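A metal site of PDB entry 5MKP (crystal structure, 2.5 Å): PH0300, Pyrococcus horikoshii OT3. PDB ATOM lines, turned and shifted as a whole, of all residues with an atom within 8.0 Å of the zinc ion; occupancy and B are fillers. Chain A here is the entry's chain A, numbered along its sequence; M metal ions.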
ATOM      1  N   LYS A   5     -18.618  14.008  13.675  1.00  0.00           N
ATOM      2  CA  LYS A   5     -17.499  14.873  13.262  1.00  0.00           C
ATOM      3  C   LYS A   5     -17.110  15.974  14.267  1.00  0.00           C
ATOM      4  O   LYS A   5     -17.958  16.452  15.035  1.00  0.00           O
ATOM      5  CB  LYS A   5     -17.773  15.494  11.870  1.00  0.00           C
ATOM      6  CG  LYS A   5     -18.011  14.466  10.756  1.00  0.00           C
ATOM      7  CD  LYS A   5     -16.721  13.769  10.300  1.00  0.00           C
ATOM      8  CE  LYS A   5     -16.972  12.545   9.444  1.00  0.00           C
ATOM      9  NZ  LYS A   5     -17.205  11.337  10.266  1.00  0.00           N
ATOM     10  N   CYS A   6     -15.809  16.394  14.221  1.00  0.00           N
ATOM     11  CA  CYS A   6     -15.216  17.449  15.041  1.00  0.00           C
ATOM     12  C   CYS A   6     -15.862  18.815  14.747  1.00  0.00           C
ATOM     13  O   CYS A   6     -16.249  19.109  13.610  1.00  0.00           O
ATOM     14  CB  CYS A   6     -13.701  17.504  14.822  1.00  0.00           C
ATOM     15  SG  CYS A   6     -12.847  18.839  15.715  1.00  0.00           S
ATOM     16  N   LYS A   7     -15.959  19.647  15.794  1.00  0.00           N
ATOM     17  CA  LYS A   7     -16.521  20.996  15.724  1.00  0.00           C
ATOM     18  C   LYS A   7     -15.624  21.949  14.896  1.00  0.00           C
ATOM     19  O   LYS A   7     -16.154  22.740  14.103  1.00  0.00           O
ATOM     20  CB  LYS A   7     -16.715  21.536  17.158  1.00  0.00           C
ATOM     21  CG  LYS A   7     -17.440  22.864  17.238  1.00  0.00           C
ATOM     22  CD  LYS A   7     -17.076  23.586  18.514  1.00  0.00           C
ATOM     23  CE  LYS A   7     -17.972  24.770  18.751  1.00  0.00           C
ATOM     24  NZ  LYS A   7     -17.407  25.697  19.760  1.00  0.00           N
ATOM     25  N   PHE A   8     -14.294  21.865  15.061  1.00  0.00           N
ATOM     26  CA  PHE A   8     -13.328  22.737  14.376  1.00  0.00           C
ATOM     27  C   PHE A   8     -12.777  22.195  13.050  1.00  0.00           C
ATOM     28  O   PHE A   8     -12.160  22.971  12.309  1.00  0.00           O
ATOM     29  CB  PHE A   8     -12.175  23.118  15.324  1.00  0.00           C
ATOM     30  CG  PHE A   8     -12.683  23.853  16.541  1.00  0.00           C
ATOM     31  CD1 PHE A   8     -12.961  25.211  16.494  1.00  0.00           C
ATOM     32  CD2 PHE A   8     -12.931  23.166  17.737  1.00  0.00           C
ATOM     33  CE1 PHE A   8     -13.453  25.875  17.621  1.00  0.00           C
ATOM     34  CE2 PHE A   8     -13.429  23.838  18.856  1.00  0.00           C
ATOM     35  CZ  PHE A   8     -13.695  25.187  18.790  1.00  0.00           C
ATOM     36  N   CYS A   9     -13.023  20.905  12.720  1.00  0.00           N
ATOM     37  CA  CYS A   9     -12.580  20.334  11.447  1.00  0.00           C
ATOM     38  C   CYS A   9     -13.529  19.240  10.900  1.00  0.00           C
ATOM     39  O   CYS A   9     -14.581  18.999  11.500  1.00  0.00           O
ATOM     40  CB  CYS A   9     -11.126  19.857  11.515  1.00  0.00           C
ATOM     41  SG  CYS A   9     -10.918  18.282  12.385  1.00  0.00           S
ATOM     42  N   SER A  10     -13.160  18.603   9.758  1.00  0.00           N
ATOM     43  CA  SER A  10     -13.917  17.565   9.074  1.00  0.00           C
ATOM     44  C   SER A  10     -13.493  16.151   9.500  1.00  0.00           C
ATOM     45  O   SER A  10     -14.042  15.158   8.997  1.00  0.00           O
ATOM     46  CB  SER A  10     -13.798  17.749   7.563  1.00  0.00           C
ATOM     47  OG  SER A  10     -14.653  16.871   6.845  1.00  0.00           O
ATOM     48  N   ARG A  11     -12.517  16.041  10.434  1.00  0.00           N
ATOM     49  CA  ARG A  11     -12.014  14.767  10.939  1.00  0.00           C
ATOM     50  C   ARG A  11     -13.053  14.145  11.882  1.00  0.00           C
ATOM     51  O   ARG A  11     -13.887  14.871  12.435  1.00  0.00           O
ATOM     52  CB  ARG A  11     -10.671  14.941  11.679  1.00  0.00           C
ATOM     53  CG  ARG A  11      -9.486  15.247  10.787  1.00  0.00           C
ATOM     54  CD  ARG A  11      -8.284  15.699  11.585  1.00  0.00           C
ATOM     55  NE  ARG A  11      -7.235  16.234  10.716  1.00  0.00           N
ATOM     56  CZ  ARG A  11      -7.056  17.531  10.459  1.00  0.00           C
ATOM     57  NH1 ARG A  11      -7.839  18.443  11.020  1.00  0.00           N
ATOM     58  NH2 ARG A  11      -6.081  17.919   9.642  1.00  0.00           N
ATOM     59  N   GLU A  12     -13.010  12.797  12.065  1.00  0.00           N
ATOM     60  CA  GLU A  12     -13.904  12.047  12.957  1.00  0.00           C
ATOM     61  C   GLU A  12     -13.716  12.496  14.404  1.00  0.00           C
ATOM     62  O   GLU A  12     -12.590  12.769  14.809  1.00  0.00           O
ATOM     63  CB  GLU A  12     -13.640  10.523  12.859  1.00  0.00           C
ATOM     64  CG  GLU A  12     -14.536   9.794  11.852  1.00  0.00           C
ATOM     65  CD  GLU A  12     -14.058   9.734  10.409  1.00  0.00           C
ATOM     66  OE1 GLU A  12     -12.849   9.507  10.172  1.00  0.00           O
ATOM     67  OE2 GLU A  12     -14.916   9.847   9.503  1.00  0.00           O
ATOM     68  N   ALA A  13     -14.818  12.586  15.165  1.00  0.00           N
ATOM     69  CA  ALA A  13     -14.775  12.979  16.572  1.00  0.00           C
ATOM     70  C   ALA A  13     -14.161  11.855  17.411  1.00  0.00           C
ATOM     71  O   ALA A  13     -14.421  10.667  17.179  1.00  0.00           O
ATOM     72  CB  ALA A  13     -16.167  13.325  17.069  1.00  0.00           C
ATOM     73  N   TYR A  14     -13.284  12.238  18.331  1.00  0.00           N
ATOM     74  CA  TYR A  14     -12.591  11.315  19.220  1.00  0.00           C
ATOM     75  C   TYR A  14     -13.293  11.189  20.566  1.00  0.00           C
ATOM     76  O   TYR A  14     -13.453  10.091  21.084  1.00  0.00           O
ATOM     77  CB  TYR A  14     -11.131  11.777  19.390  1.00  0.00           C
ATOM     78  CG  TYR A  14     -10.306  11.031  20.402  1.00  0.00           C
ATOM     79  CD1 TYR A  14     -10.043   9.676  20.252  1.00  0.00           C
ATOM     80  CD2 TYR A  14      -9.671  11.704  21.448  1.00  0.00           C
ATOM     81  CE1 TYR A  14      -9.250   8.984  21.172  1.00  0.00           C
ATOM     82  CE2 TYR A  14      -8.870  11.023  22.361  1.00  0.00           C
ATOM     83  CZ  TYR A  14      -8.652   9.664  22.218  1.00  0.00           C
ATOM     84  OH  TYR A  14      -7.867   8.971  23.107  1.00  0.00           O
ATOM     85  N   TYR A  23     -17.874  18.251  20.127  1.00  0.00           N
ATOM     86  CA  TYR A  23     -17.263  16.994  19.716  1.00  0.00           C
ATOM     87  C   TYR A  23     -15.918  17.404  19.118  1.00  0.00           C
ATOM     88  O   TYR A  23     -15.841  18.325  18.284  1.00  0.00           O
ATOM     89  CB  TYR A  23     -18.138  16.266  18.670  1.00  0.00           C
ATOM     90  CG  TYR A  23     -19.258  15.436  19.262  1.00  0.00           C
ATOM     91  CD1 TYR A  23     -19.048  14.120  19.656  1.00  0.00           C
ATOM     92  CD2 TYR A  23     -20.545  15.965  19.404  1.00  0.00           C
ATOM     93  CE1 TYR A  23     -20.084  13.336  20.162  1.00  0.00           C
ATOM     94  CE2 TYR A  23     -21.586  15.201  19.923  1.00  0.00           C
ATOM     95  CZ  TYR A  23     -21.357  13.886  20.292  1.00  0.00           C
ATOM     96  OH  TYR A  23     -22.379  13.124  20.822  1.00  0.00           O
ATOM     97  N   LEU A  24     -14.849  16.769  19.599  1.00  0.00           N
ATOM     98  CA  LEU A  24     -13.502  17.103  19.153  1.00  0.00           C
ATOM     99  C   LEU A  24     -12.775  15.896  18.634  1.00  0.00           C
ATOM    100  O   LEU A  24     -12.860  14.806  19.209  1.00  0.00           O
ATOM    101  CB  LEU A  24     -12.680  17.738  20.305  1.00  0.00           C
ATOM    102  CG  LEU A  24     -13.181  19.051  20.915  1.00  0.00           C
ATOM    103  CD1 LEU A  24     -12.346  19.426  22.107  1.00  0.00           C
ATOM    104  CD2 LEU A  24     -13.159  20.193  19.904  1.00  0.00           C
ATOM    105  N   CYS A  25     -11.996  16.107  17.567  1.00  0.00           N
ATOM    106  CA  CYS A  25     -11.137  15.091  16.963  1.00  0.00           C
ATOM    107  C   CYS A  25      -9.921  14.924  17.884  1.00  0.00           C
ATOM    108  O   CYS A  25      -9.709  15.733  18.793  1.00  0.00           O
ATOM    109  CB  CYS A  25     -10.731  15.518  15.560  1.00  0.00           C
ATOM    110  SG  CYS A  25      -9.567  16.899  15.518  1.00  0.00           S
ATOM    111  N   GLU A  26      -9.104  13.894  17.638  1.00  0.00           N
ATOM    112  CA  GLU A  26      -7.901  13.592  18.422  1.00  0.00           C
ATOM    113  C   GLU A  26      -6.986  14.804  18.616  1.00  0.00           C
ATOM    114  O   GLU A  26      -6.499  15.042  19.731  1.00  0.00           O
ATOM    115  CB  GLU A  26      -7.128  12.474  17.716  1.00  0.00           C
ATOM    116  CG  GLU A  26      -6.774  11.317  18.616  1.00  0.00           C
ATOM    117  CD  GLU A  26      -6.254  10.122  17.836  1.00  0.00           C
ATOM    118  OE1 GLU A  26      -5.019  10.009  17.668  1.00  0.00           O
ATOM    119  OE2 GLU A  26      -7.092   9.322  17.344  1.00  0.00           O
ATOM    120  N   GLU A  27      -6.738  15.565  17.534  1.00  0.00           N
ATOM    121  CA  GLU A  27      -5.818  16.693  17.586  1.00  0.00           C
ATOM    122  C   GLU A  27      -6.395  17.929  18.219  1.00  0.00           C
ATOM    123  O   GLU A  27      -5.671  18.632  18.921  1.00  0.00           O
ATOM    124  CB  GLU A  27      -5.209  16.990  16.214  1.00  0.00           C
ATOM    125  CG  GLU A  27      -3.989  16.129  15.919  1.00  0.00           C
ATOM    126  CD  GLU A  27      -2.724  16.367  16.731  1.00  0.00           C
ATOM    127  OE1 GLU A  27      -2.707  17.285  17.583  1.00  0.00           O
ATOM    128  OE2 GLU A  27      -1.744  15.634  16.492  1.00  0.00           O
ATOM    129  N   HIS A  28      -7.699  18.176  18.021  1.00  0.00           N
ATOM    130  CA  HIS A  28      -8.388  19.300  18.656  1.00  0.00           C
ATOM    131  C   HIS A  28      -8.652  19.060  20.126  1.00  0.00           C
ATOM    132  O   HIS A  28      -8.797  20.010  20.890  1.00  0.00           O
ATOM    133  CB  HIS A  28      -9.660  19.706  17.909  1.00  0.00           C
ATOM    134  CG  HIS A  28      -9.352  20.612  16.773  1.00  0.00           C
ATOM    135  ND1 HIS A  28      -9.410  20.171  15.479  1.00  0.00           N
ATOM    136  CD2 HIS A  28      -8.910  21.883  16.787  1.00  0.00           C
ATOM    137  CE1 HIS A  28      -9.026  21.195  14.729  1.00  0.00           C
ATOM    138  NE2 HIS A  28      -8.716  22.251  15.475  1.00  0.00           N
ATOM    139  N   PHE A  29      -8.710  17.778  20.542  1.00  0.00           N
ATOM    140  CA  PHE A  29      -8.852  17.388  21.942  1.00  0.00           C
ATOM    141  C   PHE A  29      -7.534  17.699  22.663  1.00  0.00           C
ATOM    142  O   PHE A  29      -7.562  18.337  23.717  1.00  0.00           O
ATOM    143  CB  PHE A  29      -9.223  15.907  22.094  1.00  0.00           C
ATOM    144  CG  PHE A  29      -9.167  15.468  23.546  1.00  0.00           C
ATOM    145  CD1 PHE A  29     -10.027  16.020  24.498  1.00  0.00           C
ATOM    146  CD2 PHE A  29      -8.184  14.572  23.977  1.00  0.00           C
ATOM    147  CE1 PHE A  29      -9.917  15.664  25.844  1.00  0.00           C
ATOM    148  CE2 PHE A  29      -8.089  14.224  25.319  1.00  0.00           C
ATOM    149  CZ  PHE A  29      -8.966  14.774  26.247  1.00  0.00           C
ATOM    150  N   GLU A  31      -5.280  19.844  21.909  1.00  0.00           N
ATOM    151  CA  GLU A  31      -5.196  21.313  21.992  1.00  0.00           C
ATOM    152  C   GLU A  31      -6.072  21.808  23.144  1.00  0.00           C
ATOM    153  O   GLU A  31      -5.553  22.526  24.009  1.00  0.00           O
ATOM    154  CB  GLU A  31      -5.592  21.973  20.657  1.00  0.00           C
ATOM    155  CG  GLU A  31      -5.349  23.474  20.639  1.00  0.00           C
ATOM    156  CD  GLU A  31      -5.872  24.266  19.452  1.00  0.00           C
ATOM    157  OE1 GLU A  31      -5.159  25.200  19.008  1.00  0.00           O
ATOM    158  OE2 GLU A  31      -7.014  24.000  19.008  1.00  0.00           O
HETATM  159 ZN    ZN M   1     -10.823  18.710  14.592  1.00  0.00          ZN
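The backbone NH (N) of Cys 6 is in hydrogen-bond range of the backbone carbonyl oxygen (O) of Arg 11.
The guanidinium group (NH1) of Arg 11 lies close to the side-chain sulfur (SG) of Cys 9 (3.4 Å).
The backbone NH (N) of Phe 8 lies close to the side-chain sulfur (SG) of Cys 6 (3.4 Å).
SG of Cys 25 lies close to N of Glu 27.
Within 4 Å of the zinc ion: Cys 6, Cys 9, Cys 25 and His 28.
The zinc ion is bound by a ring nitrogen (ND1) of His 28 (2.2 Å), the side-chain sulfur of Cys 9 (2.3 Å), the side-chain sulfur of Cys 6 (2.3 Å) and the side-chain sulfur of Cys 25 (2.4 Å).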
